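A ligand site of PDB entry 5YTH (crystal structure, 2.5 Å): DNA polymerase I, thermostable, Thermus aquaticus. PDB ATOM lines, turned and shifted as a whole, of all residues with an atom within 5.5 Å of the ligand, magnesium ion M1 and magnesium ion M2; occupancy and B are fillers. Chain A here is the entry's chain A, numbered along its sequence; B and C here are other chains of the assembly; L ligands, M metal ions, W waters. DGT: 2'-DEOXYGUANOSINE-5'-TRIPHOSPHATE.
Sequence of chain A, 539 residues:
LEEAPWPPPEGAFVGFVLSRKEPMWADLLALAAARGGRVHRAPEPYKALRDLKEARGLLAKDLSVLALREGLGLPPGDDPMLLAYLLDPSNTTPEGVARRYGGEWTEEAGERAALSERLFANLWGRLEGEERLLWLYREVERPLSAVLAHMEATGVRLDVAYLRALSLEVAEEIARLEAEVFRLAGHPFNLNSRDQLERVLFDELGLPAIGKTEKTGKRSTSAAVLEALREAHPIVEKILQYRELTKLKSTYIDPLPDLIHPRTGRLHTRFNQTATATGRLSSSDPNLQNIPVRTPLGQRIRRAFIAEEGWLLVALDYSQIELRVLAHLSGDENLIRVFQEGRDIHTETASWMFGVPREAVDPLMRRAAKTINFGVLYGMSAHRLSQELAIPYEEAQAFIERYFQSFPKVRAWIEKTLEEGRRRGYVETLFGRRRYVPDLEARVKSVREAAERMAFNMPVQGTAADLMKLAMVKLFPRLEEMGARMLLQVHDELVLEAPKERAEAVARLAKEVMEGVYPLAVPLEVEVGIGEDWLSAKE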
ATOM      1  N   ARG A 280     -20.063   2.916  -7.701  1.00  0.00           N
ATOM      2  CA  ARG A 280     -18.750   2.721  -8.326  1.00  0.00           C
ATOM      3  C   ARG A 280     -18.234   3.980  -8.981  1.00  0.00           C
ATOM      4  O   ARG A 280     -19.002   4.862  -9.364  1.00  0.00           O
ATOM      5  CB  ARG A 280     -18.816   1.671  -9.437  1.00  0.00           C
ATOM      6  CG  ARG A 280     -18.867   0.243  -8.968  1.00  0.00           C
ATOM      7  CD  ARG A 280     -18.590  -0.671 -10.142  1.00  0.00           C
ATOM      8  NE  ARG A 280     -18.364  -2.050  -9.718  1.00  0.00           N
ATOM      9  CZ  ARG A 280     -17.950  -3.032 -10.523  1.00  0.00           C
ATOM     10  NH1 ARG A 280     -17.731  -2.815 -11.818  1.00  0.00           N
ATOM     11  NH2 ARG A 280     -17.763  -4.245 -10.019  1.00  0.00           N
ATOM     12  N   ASP A 317      -5.805  -6.695  -5.323  1.00  0.00           N
ATOM     13  CA  ASP A 317      -7.175  -7.003  -5.745  1.00  0.00           C
ATOM     14  C   ASP A 317      -7.894  -7.775  -4.649  1.00  0.00           C
ATOM     15  O   ASP A 317      -7.406  -8.824  -4.195  1.00  0.00           O
ATOM     16  CB  ASP A 317      -7.128  -7.840  -7.028  1.00  0.00           C
ATOM     17  CG  ASP A 317      -8.502  -8.042  -7.647  1.00  0.00           C
ATOM     18  OD1 ASP A 317      -9.372  -8.664  -7.018  1.00  0.00           O
ATOM     19  OD2 ASP A 317      -8.712  -7.589  -8.784  1.00  0.00           O
ATOM     20  N   TYR A 318      -9.057  -7.278  -4.230  1.00  0.00           N
ATOM     21  CA  TYR A 318      -9.868  -7.977  -3.241  1.00  0.00           C
ATOM     22  C   TYR A 318     -10.341  -9.329  -3.747  1.00  0.00           C
ATOM     23  O   TYR A 318     -10.801  -9.448  -4.873  1.00  0.00           O
ATOM     24  CB  TYR A 318     -11.114  -7.169  -2.876  1.00  0.00           C
ATOM     25  CG  TYR A 318     -10.870  -6.085  -1.868  1.00  0.00           C
ATOM     26  CD1 TYR A 318     -10.732  -6.395  -0.505  1.00  0.00           C
ATOM     27  CD2 TYR A 318     -10.816  -4.752  -2.253  1.00  0.00           C
ATOM     28  CE1 TYR A 318     -10.525  -5.388   0.424  1.00  0.00           C
ATOM     29  CE2 TYR A 318     -10.616  -3.748  -1.318  1.00  0.00           C
ATOM     30  CZ  TYR A 318     -10.471  -4.076   0.003  1.00  0.00           C
ATOM     31  OH  TYR A 318     -10.280  -3.064   0.889  1.00  0.00           O
ATOM     32  N   SER A 319     -10.233 -10.329  -2.895  1.00  0.00           N
ATOM     33  CA  SER A 319     -10.635 -11.678  -3.244  1.00  0.00           C
ATOM     34  C   SER A 319     -12.154 -11.831  -3.207  1.00  0.00           C
ATOM     35  O   SER A 319     -12.782 -11.450  -2.208  1.00  0.00           O
ATOM     36  CB  SER A 319      -9.978 -12.679  -2.291  1.00  0.00           C
ATOM     37  OG  SER A 319     -10.456 -13.992  -2.528  1.00  0.00           O
ATOM     38  N   GLN A 320     -12.734 -12.366  -4.284  1.00  0.00           N
ATOM     39  CA  GLN A 320     -14.135 -12.795  -4.319  1.00  0.00           C
ATOM     40  C   GLN A 320     -15.057 -11.753  -3.712  1.00  0.00           C
ATOM     41  O   GLN A 320     -15.963 -12.080  -2.939  1.00  0.00           O
ATOM     42  CB  GLN A 320     -14.291 -14.135  -3.617  1.00  0.00           C
ATOM     43  CG  GLN A 320     -13.375 -15.223  -4.175  1.00  0.00           C
ATOM     44  CD  GLN A 320     -13.502 -16.542  -3.437  1.00  0.00           C
ATOM     45  OE1 GLN A 320     -14.422 -17.326  -3.695  1.00  0.00           O
ATOM     46  NE2 GLN A 320     -12.573 -16.804  -2.527  1.00  0.00           N
ATOM     47  N   ILE A 321     -14.816 -10.501  -4.060  1.00  0.00           N
ATOM     48  CA  ILE A 321     -15.296  -9.383  -3.240  1.00  0.00           C
ATOM     49  C   ILE A 321     -16.813  -9.388  -3.032  1.00  0.00           C
ATOM     50  O   ILE A 321     -17.258  -9.452  -1.887  1.00  0.00           O
ATOM     51  CB  ILE A 321     -14.742  -7.994  -3.681  1.00  0.00           C
ATOM     52  CG1 ILE A 321     -15.270  -6.873  -2.791  1.00  0.00           C
ATOM     53  CG2 ILE A 321     -15.069  -7.657  -5.131  1.00  0.00           C
ATOM     54  CD1 ILE A 321     -14.965  -7.048  -1.317  1.00  0.00           C
ATOM     55  N   GLU A 322     -17.599  -9.381  -4.098  1.00  0.00           N
ATOM     56  CA  GLU A 322     -19.057  -9.214  -3.957  1.00  0.00           C
ATOM     57  C   GLU A 322     -19.744 -10.419  -3.304  1.00  0.00           C
ATOM     58  O   GLU A 322     -20.783 -10.251  -2.654  1.00  0.00           O
ATOM     59  CB  GLU A 322     -19.704  -8.793  -5.299  1.00  0.00           C
ATOM     60  CG  GLU A 322     -19.409  -7.319  -5.615  1.00  0.00           C
ATOM     61  CD  GLU A 322     -20.045  -6.787  -6.905  1.00  0.00           C
ATOM     62  OE1 GLU A 322     -21.203  -7.125  -7.218  1.00  0.00           O
ATOM     63  OE2 GLU A 322     -19.346  -6.004  -7.598  1.00  0.00           O
ATOM     64  N   LEU A 323     -19.141 -11.603  -3.423  1.00  0.00           N
ATOM     65  CA  LEU A 323     -19.587 -12.773  -2.667  1.00  0.00           C
ATOM     66  C   LEU A 323     -19.410 -12.580  -1.169  1.00  0.00           C
ATOM     67  O   LEU A 323     -20.340 -12.841  -0.395  1.00  0.00           O
ATOM     68  CB  LEU A 323     -18.825 -14.024  -3.102  1.00  0.00           C
ATOM     69  CG  LEU A 323     -19.069 -14.552  -4.513  1.00  0.00           C
ATOM     70  CD1 LEU A 323     -18.097 -15.684  -4.830  1.00  0.00           C
ATOM     71  CD2 LEU A 323     -20.511 -15.005  -4.683  1.00  0.00           C
ATOM     72  N   ASP A 344     -12.185 -20.978  -2.270  1.00  0.00           N
ATOM     73  CA  ASP A 344     -12.398 -20.164  -3.479  1.00  0.00           C
ATOM     74  C   ASP A 344     -13.517 -20.739  -4.346  1.00  0.00           C
ATOM     75  O   ASP A 344     -13.385 -21.826  -4.917  1.00  0.00           O
ATOM     76  CB  ASP A 344     -11.100 -20.044  -4.277  1.00  0.00           C
ATOM     77  CG  ASP A 344     -11.137 -18.879  -5.274  1.00  0.00           C
ATOM     78  OD1 ASP A 344     -12.190 -18.643  -5.911  1.00  0.00           O
ATOM     79  OD2 ASP A 344     -10.089 -18.216  -5.426  1.00  0.00           O
ATOM     80  N   HIS A 346     -14.779 -19.318  -7.164  1.00  0.00           N
ATOM     81  CA  HIS A 346     -14.403 -19.214  -8.578  1.00  0.00           C
ATOM     82  C   HIS A 346     -13.535 -20.383  -9.024  1.00  0.00           C
ATOM     83  O   HIS A 346     -13.642 -20.830 -10.156  1.00  0.00           O
ATOM     84  CB  HIS A 346     -13.687 -17.884  -8.868  1.00  0.00           C
ATOM     85  CG  HIS A 346     -14.497 -16.660  -8.547  1.00  0.00           C
ATOM     86  ND1 HIS A 346     -15.866 -16.673  -8.413  1.00  0.00           N
ATOM     87  CD2 HIS A 346     -14.116 -15.371  -8.354  1.00  0.00           C
ATOM     88  CE1 HIS A 346     -16.289 -15.456  -8.136  1.00  0.00           C
ATOM     89  NE2 HIS A 346     -15.252 -14.649  -8.102  1.00  0.00           N
ATOM     90  N   ARG A 366     -10.975 -19.458 -14.778  1.00  0.00           N
ATOM     91  CA  ARG A 366     -11.423 -18.714 -13.601  1.00  0.00           C
ATOM     92  C   ARG A 366     -12.351 -17.560 -14.012  1.00  0.00           C
ATOM     93  O   ARG A 366     -13.390 -17.350 -13.389  1.00  0.00           O
ATOM     94  CB  ARG A 366     -10.205 -18.219 -12.812  1.00  0.00           C
ATOM     95  CG  ARG A 366     -10.524 -17.781 -11.390  1.00  0.00           C
ATOM     96  CD  ARG A 366      -9.275 -17.766 -10.485  1.00  0.00           C
ATOM     97  NE  ARG A 366      -9.681 -17.455  -9.123  1.00  0.00           N
ATOM     98  CZ  ARG A 366     -10.022 -16.241  -8.696  1.00  0.00           C
ATOM     99  NH1 ARG A 366      -9.968 -15.193  -9.502  1.00  0.00           N
ATOM    100  NH2 ARG A 366     -10.415 -16.085  -7.434  1.00  0.00           N
ATOM    101  N   ARG A 367     -11.982 -16.842 -15.079  1.00  0.00           N
ATOM    102  CA  ARG A 367     -12.813 -15.738 -15.587  1.00  0.00           C
ATOM    103  C   ARG A 367     -14.177 -16.246 -16.033  1.00  0.00           C
ATOM    104  O   ARG A 367     -15.210 -15.712 -15.619  1.00  0.00           O
ATOM    105  CB  ARG A 367     -12.070 -15.010 -16.733  1.00  0.00           C
ATOM    106  CG  ARG A 367     -12.773 -13.815 -17.373  1.00  0.00           C
ATOM    107  CD  ARG A 367     -13.365 -12.814 -16.387  1.00  0.00           C
ATOM    108  NE  ARG A 367     -14.784 -13.049 -16.094  1.00  0.00           N
ATOM    109  CZ  ARG A 367     -15.584 -12.197 -15.453  1.00  0.00           C
ATOM    110  NH1 ARG A 367     -16.864 -12.519 -15.258  1.00  0.00           N
ATOM    111  NH2 ARG A 367     -15.139 -11.014 -15.006  1.00  0.00           N
ATOM    112  N   LYS A 370     -16.387 -16.960 -13.079  1.00  0.00           N
ATOM    113  CA  LYS A 370     -16.992 -15.781 -12.430  1.00  0.00           C
ATOM    114  C   LYS A 370     -18.349 -15.454 -13.056  1.00  0.00           C
ATOM    115  O   LYS A 370     -19.333 -15.235 -12.334  1.00  0.00           O
ATOM    116  CB  LYS A 370     -16.094 -14.545 -12.535  1.00  0.00           C
ATOM    117  CG  LYS A 370     -14.690 -14.747 -11.991  1.00  0.00           C
ATOM    118  CD  LYS A 370     -14.026 -13.441 -11.589  1.00  0.00           C
ATOM    119  CE  LYS A 370     -12.519 -13.613 -11.454  1.00  0.00           C
ATOM    120  NZ  LYS A 370     -11.863 -12.342 -11.059  1.00  0.00           N
ATOM    121  N   THR A 371     -18.371 -15.421 -14.393  1.00  0.00           N
ATOM    122  CA  THR A 371     -19.617 -15.224 -15.160  1.00  0.00           C
ATOM    123  C   THR A 371     -20.724 -16.176 -14.709  1.00  0.00           C
ATOM    124  O   THR A 371     -21.862 -15.754 -14.538  1.00  0.00           O
ATOM    125  CB  THR A 371     -19.397 -15.473 -16.666  1.00  0.00           C
ATOM    126  OG1 THR A 371     -18.217 -14.803 -17.106  1.00  0.00           O
ATOM    127  CG2 THR A 371     -20.586 -14.978 -17.486  1.00  0.00           C
ATOM    128  N   PHE A 374     -21.586 -15.104 -10.657  1.00  0.00           N
ATOM    129  CA  PHE A 374     -22.294 -13.820 -10.518  1.00  0.00           C
ATOM    130  C   PHE A 374     -23.581 -13.797 -11.330  1.00  0.00           C
ATOM    131  O   PHE A 374     -24.614 -13.327 -10.853  1.00  0.00           O
ATOM    132  CB  PHE A 374     -21.384 -12.642 -10.891  1.00  0.00           C
ATOM    133  CG  PHE A 374     -20.211 -12.462  -9.972  1.00  0.00           C
ATOM    134  CD1 PHE A 374     -20.415 -12.334  -8.594  1.00  0.00           C
ATOM    135  CD2 PHE A 374     -18.914 -12.419 -10.467  1.00  0.00           C
ATOM    136  CE1 PHE A 374     -19.347 -12.193  -7.734  1.00  0.00           C
ATOM    137  CE2 PHE A 374     -17.833 -12.274  -9.592  1.00  0.00           C
ATOM    138  CZ  PHE A 374     -18.063 -12.154  -8.229  1.00  0.00           C
ATOM    139  N   GLY A 375     -23.501 -14.313 -12.566  1.00  0.00           N
ATOM    140  CA  GLY A 375     -24.665 -14.542 -13.423  1.00  0.00           C
ATOM    141  C   GLY A 375     -25.833 -15.178 -12.700  1.00  0.00           C
ATOM    142  O   GLY A 375     -26.911 -14.584 -12.625  1.00  0.00           O
ATOM    143  N   TYR A 378     -27.215 -12.936  -9.695  1.00  0.00           N
ATOM    144  CA  TYR A 378     -27.923 -11.724 -10.087  1.00  0.00           C
ATOM    145  C   TYR A 378     -29.119 -11.943 -11.028  1.00  0.00           C
ATOM    146  O   TYR A 378     -29.839 -10.991 -11.325  1.00  0.00           O
ATOM    147  CB  TYR A 378     -26.923 -10.682 -10.609  1.00  0.00           C
ATOM    148  CG  TYR A 378     -25.993 -10.199  -9.513  1.00  0.00           C
ATOM    149  CD1 TYR A 378     -26.503  -9.638  -8.333  1.00  0.00           C
ATOM    150  CD2 TYR A 378     -24.603 -10.327  -9.619  1.00  0.00           C
ATOM    151  CE1 TYR A 378     -25.677  -9.214  -7.317  1.00  0.00           C
ATOM    152  CE2 TYR A 378     -23.765  -9.898  -8.603  1.00  0.00           C
ATOM    153  CZ  TYR A 378     -24.317  -9.342  -7.452  1.00  0.00           C
ATOM    154  OH  TYR A 378     -23.522  -8.897  -6.429  1.00  0.00           O
ATOM    155  N   ASN A 457     -28.895  -6.072  -6.926  1.00  0.00           N
ATOM    156  CA  ASN A 457     -27.467  -5.962  -7.241  1.00  0.00           C
ATOM    157  C   ASN A 457     -26.796  -4.793  -6.536  1.00  0.00           C
ATOM    158  O   ASN A 457     -25.689  -4.923  -6.025  1.00  0.00           O
ATOM    159  CB  ASN A 457     -27.251  -5.829  -8.756  1.00  0.00           C
ATOM    160  CG  ASN A 457     -25.798  -5.539  -9.125  1.00  0.00           C
ATOM    161  OD1 ASN A 457     -25.437  -4.392  -9.381  1.00  0.00           O
ATOM    162  ND2 ASN A 457     -24.978  -6.580  -9.168  1.00  0.00           N
ATOM    163  N   VAL A 490      -9.407  -0.017 -10.092  1.00  0.00           N
ATOM    164  CA  VAL A 490     -10.179  -0.815 -11.048  1.00  0.00           C
ATOM    165  C   VAL A 490     -11.216  -1.585 -10.247  1.00  0.00           C
ATOM    166  O   VAL A 490     -11.177  -2.807 -10.149  1.00  0.00           O
ATOM    167  CB  VAL A 490      -9.277  -1.746 -11.894  1.00  0.00           C
ATOM    168  CG1 VAL A 490     -10.051  -2.342 -13.067  1.00  0.00           C
ATOM    169  CG2 VAL A 490      -8.077  -0.983 -12.438  1.00  0.00           C
ATOM    170  N   ASP A 492     -12.301  -3.173  -7.597  1.00  0.00           N
ATOM    171  CA  ASP A 492     -11.874  -3.834  -6.354  1.00  0.00           C
ATOM    172  C   ASP A 492     -10.381  -4.064  -6.340  1.00  0.00           C
ATOM    173  O   ASP A 492      -9.883  -4.909  -5.600  1.00  0.00           O
ATOM    174  CB  ASP A 492     -12.611  -5.161  -6.156  1.00  0.00           C
ATOM    175  CG  ASP A 492     -12.018  -6.280  -6.981  1.00  0.00           C
ATOM    176  OD1 ASP A 492     -11.635  -6.046  -8.153  1.00  0.00           O
ATOM    177  OD2 ASP A 492     -11.927  -7.400  -6.450  1.00  0.00           O
ATOM    178  N   GLU A 493      -9.674  -3.277  -7.139  1.00  0.00           N
ATOM    179  CA  GLU A 493      -8.250  -3.371  -7.272  1.00  0.00           C
ATOM    180  C   GLU A 493      -7.654  -1.981  -7.196  1.00  0.00           C
ATOM    181  O   GLU A 493      -8.282  -1.005  -7.611  1.00  0.00           O
ATOM    182  CB  GLU A 493      -7.900  -4.022  -8.612  1.00  0.00           C
ATOM    183  CG  GLU A 493      -6.464  -3.822  -9.117  1.00  0.00           C
ATOM    184  CD  GLU A 493      -6.248  -4.372 -10.520  1.00  0.00           C
ATOM    185  OE1 GLU A 493      -7.240  -4.838 -11.136  1.00  0.00           O
ATOM    186  OE2 GLU A 493      -5.090  -4.359 -11.004  1.00  0.00           O
ATOM    187  N   LYS A 538       0.111  -8.692 -11.152  1.00  0.00           N
ATOM    188  CA  LYS A 538      -1.002  -9.561 -10.749  1.00  0.00           C
ATOM    189  C   LYS A 538      -0.649 -11.061 -10.706  1.00  0.00           C
ATOM    190  O   LYS A 538      -1.276 -11.797  -9.941  1.00  0.00           O
ATOM    191  CB  LYS A 538      -2.234  -9.336 -11.622  1.00  0.00           C
ATOM    192  CG  LYS A 538      -3.119  -8.205 -11.134  1.00  0.00           C
ATOM    193  CD  LYS A 538      -4.582  -8.581 -11.297  1.00  0.00           C
ATOM    194  CE  LYS A 538      -5.470  -7.385 -11.063  1.00  0.00           C
ATOM    195  NZ  LYS A 538      -6.893  -7.771 -10.829  1.00  0.00           N
ATOM    196  P    DC B   4     -29.749 -13.505 -19.079  1.00  0.00           P
ATOM    197  OP1  DC B   4     -29.071 -13.268 -20.380  1.00  0.00           O
ATOM    198  OP2  DC B   4     -30.279 -14.851 -18.772  1.00  0.00           O
ATOM    199  O5'  DC B   4     -28.740 -13.057 -17.932  1.00  0.00           O
ATOM    200  C5'  DC B   4     -28.491 -11.657 -17.642  1.00  0.00           C
ATOM    201  C4'  DC B   4     -28.558 -11.415 -16.161  1.00  0.00           C
ATOM    202  O4'  DC B   4     -27.695 -12.328 -15.438  1.00  0.00           O
ATOM    203  C3'  DC B   4     -28.108 -10.017 -15.733  1.00  0.00           C
ATOM    204  O3'  DC B   4     -29.240  -9.155 -15.627  1.00  0.00           O
ATOM    205  C2'  DC B   4     -27.494 -10.248 -14.368  1.00  0.00           C
ATOM    206  C1'  DC B   4     -26.835 -11.603 -14.566  1.00  0.00           C
ATOM    207  N1   DC B   4     -25.488 -11.584 -15.166  1.00  0.00           N
ATOM    208  C2   DC B   4     -24.416 -11.057 -14.421  1.00  0.00           C
ATOM    209  O2   DC B   4     -24.633 -10.612 -13.287  1.00  0.00           O
ATOM    210  N3   DC B   4     -23.177 -11.056 -14.960  1.00  0.00           N
ATOM    211  C4   DC B   4     -22.978 -11.550 -16.186  1.00  0.00           C
ATOM    212  N4   DC B   4     -21.743 -11.520 -16.689  1.00  0.00           N
ATOM    213  C5   DC B   4     -24.046 -12.086 -16.960  1.00  0.00           C
ATOM    214  C6   DC B   4     -25.268 -12.091 -16.421  1.00  0.00           C
ATOM    215  P    DG B   5     -29.165  -7.664 -16.166  1.00  0.00           P
ATOM    216  OP1  DG B   5     -30.514  -7.074 -16.053  1.00  0.00           O
ATOM    217  OP2  DG B   5     -28.431  -7.684 -17.463  1.00  0.00           O
ATOM    218  O5'  DG B   5     -28.241  -6.917 -15.109  1.00  0.00           O
ATOM    219  C5'  DG B   5     -28.736  -6.607 -13.790  1.00  0.00           C
ATOM    220  C4'  DG B   5     -27.623  -6.034 -12.945  1.00  0.00           C
ATOM    221  O4'  DG B   5     -26.533  -6.976 -12.904  1.00  0.00           O
ATOM    222  C3'  DG B   5     -27.009  -4.760 -13.499  1.00  0.00           C
ATOM    223  O3'  DG B   5     -27.721  -3.608 -13.036  1.00  0.00           O
ATOM    224  C2'  DG B   5     -25.601  -4.791 -12.946  1.00  0.00           C
ATOM    225  C1'  DG B   5     -25.298  -6.278 -12.847  1.00  0.00           C
ATOM    226  N9   DG B   5     -24.445  -6.778 -13.914  1.00  0.00           N
ATOM    227  C8   DG B   5     -24.798  -7.496 -15.040  1.00  0.00           C
ATOM    228  N7   DG B   5     -23.782  -7.800 -15.791  1.00  0.00           N
ATOM    229  C5   DG B   5     -22.689  -7.244 -15.130  1.00  0.00           C
ATOM    230  C6   DG B   5     -21.310  -7.246 -15.475  1.00  0.00           C
ATOM    231  O6   DG B   5     -20.761  -7.763 -16.456  1.00  0.00           O
ATOM    232  N1   DG B   5     -20.550  -6.580 -14.521  1.00  0.00           N
ATOM    233  C2   DG B   5     -21.049  -5.982 -13.390  1.00  0.00           C
ATOM    234  N2   DG B   5     -20.159  -5.373 -12.590  1.00  0.00           N
ATOM    235  N3   DG B   5     -22.328  -5.964 -13.071  1.00  0.00           N
ATOM    236  C4   DG B   5     -23.082  -6.607 -13.982  1.00  0.00           C
ATOM    237  N1  DOC C  12     -15.626  -6.033 -13.897  1.00  0.00           N
ATOM    238  C2  DOC C  12     -17.012  -6.052 -13.898  1.00  0.00           C
ATOM    239  N3  DOC C  12     -17.667  -6.852 -14.697  1.00  0.00           N
ATOM    240  C4  DOC C  12     -17.024  -7.633 -15.538  1.00  0.00           C
ATOM    241  C5  DOC C  12     -15.669  -7.647 -15.580  1.00  0.00           C
ATOM    242  C6  DOC C  12     -14.986  -6.826 -14.745  1.00  0.00           C
ATOM    243  O2  DOC C  12     -17.659  -5.358 -13.150  1.00  0.00           O
ATOM    244  N4  DOC C  12     -17.711  -8.423 -16.351  1.00  0.00           N
ATOM    245  C1' DOC C  12     -14.884  -5.149 -13.011  1.00  0.00           C
ATOM    246  C2' DOC C  12     -14.509  -5.852 -11.734  1.00  0.00           C
ATOM    247  C3' DOC C  12     -13.059  -6.202 -11.906  1.00  0.00           C
ATOM    248  C4' DOC C  12     -12.572  -5.154 -12.853  1.00  0.00           C
ATOM    249  O4' DOC C  12     -13.678  -4.766 -13.630  1.00  0.00           O
ATOM    250  C5' DOC C  12     -11.432  -5.646 -13.725  1.00  0.00           C
ATOM    251  O5' DOC C  12     -11.733  -6.774 -14.487  1.00  0.00           O
ATOM    252  P   DOC C  12     -10.572  -7.514 -15.227  1.00  0.00           P
ATOM    253  OP1 DOC C  12      -9.373  -7.378 -14.442  1.00  0.00           O
ATOM    254  OP2 DOC C  12     -11.055  -8.829 -15.542  1.00  0.00           O
HETATM  255  PG  DGT L   1     -11.099 -12.404  -7.610  1.00  0.00           P
HETATM  256  O1G DGT L   1     -10.996 -13.386  -6.468  1.00  0.00           O
HETATM  257  O2G DGT L   1     -10.442 -12.868  -8.872  1.00  0.00           O
HETATM  258  O3G DGT L   1     -10.684 -11.008  -7.260  1.00  0.00           O
HETATM  259  O3B DGT L   1     -12.684 -12.441  -7.898  1.00  0.00           O
HETATM  260  PB  DGT L   1     -13.688 -11.212  -7.736  1.00  0.00           P
HETATM  261  O1B DGT L   1     -15.050 -11.768  -7.433  1.00  0.00           O
HETATM  262  O2B DGT L   1     -13.183 -10.181  -6.753  1.00  0.00           O
HETATM  263  O3A DGT L   1     -13.686 -10.679  -9.257  1.00  0.00           O
HETATM  264  PA  DGT L   1     -12.922  -9.383  -9.801  1.00  0.00           P
HETATM  265  O1A DGT L   1     -12.390  -9.669 -11.175  1.00  0.00           O
HETATM  266  O2A DGT L   1     -11.918  -8.872  -8.809  1.00  0.00           O
HETATM  267  O5' DGT L   1     -14.140  -8.360  -9.878  1.00  0.00           O
HETATM  268  C5' DGT L   1     -14.561  -7.627  -8.737  1.00  0.00           C
HETATM  269  C4' DGT L   1     -16.070  -7.650  -8.571  1.00  0.00           C
HETATM  270  O4' DGT L   1     -16.736  -7.045  -9.677  1.00  0.00           O
HETATM  271  C3' DGT L   1     -16.649  -9.056  -8.449  1.00  0.00           C
HETATM  272  O3' DGT L   1     -16.548  -9.571  -7.125  1.00  0.00           O
HETATM  273  C2' DGT L   1     -18.075  -8.799  -8.865  1.00  0.00           C
HETATM  274  C1' DGT L   1     -17.957  -7.726  -9.932  1.00  0.00           C
HETATM  275  N9  DGT L   1     -17.938  -8.488 -11.200  1.00  0.00           N
HETATM  276  C8  DGT L   1     -16.874  -8.945 -11.889  1.00  0.00           C
HETATM  277  N7  DGT L   1     -17.272  -9.627 -12.972  1.00  0.00           N
HETATM  278  C5  DGT L   1     -18.619  -9.631 -12.972  1.00  0.00           C
HETATM  279  C6  DGT L   1     -19.685 -10.187 -13.824  1.00  0.00           C
HETATM  280  O6  DGT L   1     -19.388 -10.838 -14.839  1.00  0.00           O
HETATM  281  N1  DGT L   1     -20.958  -9.964 -13.453  1.00  0.00           N
HETATM  282  C2  DGT L   1     -21.287  -9.251 -12.346  1.00  0.00           C
HETATM  283  N2  DGT L   1     -22.582  -9.047 -12.018  1.00  0.00           N
HETATM  284  N3  DGT L   1     -20.350  -8.711 -11.525  1.00  0.00           N
HETATM  285  C4  DGT L   1     -19.040  -8.878 -11.796  1.00  0.00           C
HETATM  286 MG    MG M   1     -11.465  -9.337  -6.806  1.00  0.00          MG
HETATM  287 MG    MG M   2     -10.604  -7.296  -9.914  1.00  0.00          MG
HETATM  288  O   HOH W   1      -9.720  -8.450 -11.781  1.00  0.00           O
HETATM  289  O   HOH W   2      -8.134 -11.221  -5.864  1.00  0.00           O
HETATM  290  O   HOH W   3     -10.060  -5.463 -10.490  1.00  0.00           O
HETATM  291  O   HOH W   4     -21.957  -6.744  -9.920  1.00  0.00           O
HETATM  292  O   HOH W   5      -9.059 -10.512  -9.739  1.00  0.00           O
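Water W1 lies within hydrogen-bond range of OP1 of DOC 12 of chain C (2.9 Å), O1A of the ligand (3.0 Å) and NZ of Lys 538 (3.1 Å). Water W3 bridges O of Val 490 (2.9 Å) and OE1 of Glu 493 (3.0 Å).
The backbone NH (N) of His 346 is in hydrogen-bond range of the side-chain carboxylate (OD1) of Asp 344 (3.0 Å). The side-chain carboxylate (OD1) of Asp 344 lies close to the side-chain amide oxygen (OE1) of Gln 320, at 3.4 Å. O2 of DOC 12 of chain C lies close to N2 of DG 5 of chain B, at 2.6 Å. OD2 of Asp 344 lies within salt-bridge range of NH2 of Arg 366 (2.9 Å). The side-chain hydroxyl (OG1) of Thr 371 sits at hydrogen-bond distance from the guanidinium group (NH1) of Arg 367, at 3.2 Å. O2 of DOC 12 of chain C is in hydrogen-bond range of NH1 of Arg 280, at 2.9 Å. The side-chain carboxylate of Glu 322 is in salt-bridge range of the guanidinium group of Arg 280. The side-chain amino group (NZ) of Lys 538 is in salt-bridge range of the side-chain carboxylate (OE1) of Glu 493, 3.0 Å away.
The guanidinium group (NH2) of Arg 280 sits at hydrogen-bond distance from an oxygen (O4') of the ligand (3.0 Å). NE2 of His 346 is in hydrogen-bond range of O1B of the ligand, 3.0 Å away. An oxygen (O6) of the ligand lies within hydrogen-bond range of the guanidinium group (NH1) of Arg 367, 3.1 Å away. An oxygen (O2B) of the ligand lies close to the backbone NH of Ile 321 (3.2 Å). The backbone NH (N) of Gln 320 lies within hydrogen-bond range of an oxygen (O1G) of the ligand (3.0 Å). O3' of the ligand sits at hydrogen-bond distance from N of Glu 322. N2 of the ligand lies within hydrogen-bond range of O2 of DC 4 of chain B (2.9 Å). An oxygen (O2G) of the ligand lies within salt-bridge range of the side-chain amino group (NZ) of Lys 370 (2.7 Å). A nitrogen (N2) of the ligand lies close to N3 of DG 5 of chain B (3.3 Å). O2G of the ligand is in salt-bridge range of NH1 of Arg 366 (2.5 Å).
Magnesium ion M1 is bound by O3G of the ligand (1.9 Å), O2B of the ligand (1.9 Å), OD2 of Asp 492 (2.0 Å), O of Tyr 318 (2.0 Å), O2A of the ligand (2.1 Å) and OD1 of Asp 317 (2.2 Å). Magnesium ion M1 has six donor atoms within binding distance.
Residues that only touch magnesium ion M2: Lys 538 (3.9 Å) and DOC 12 of chain C (3.3 Å). Along chain A the residues within 4 Å of magnesium ion M2 span positions 317 to 538. The nearest printed residue that does not touch magnesium ion M2 is Glu 493 (4.3 Å).
N3 of DOC 12 of chain C sits close to a nitrogen (N7) of the ligand. Merely in contact with the ligand: Phe 374, Tyr 378 and Ser 319. Hydrophobic or aromatic side chains that line the ligand: Ile 321, His 346, Phe 374 and Tyr 378. Of the 25 residues printed, 17 come within 4 Å of the ligand. The nearest printed residue that does not touch the ligand is Thr 371 (4.4 Å).
Magnesium ion M2 is bound by water W3 (2.0 Å), the side-chain carboxylate (OD2) of Asp 317 (2.2 Å), an oxygen (O2A) of the ligand (2.3 Å), water W1 (2.4 Å) and the side-chain carboxylate (OD1) of Asp 492 (2.4 Å).
Three residues have an atom within 4 Å of magnesium ion M1: Asp 317, Tyr 318 and Asp 492.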
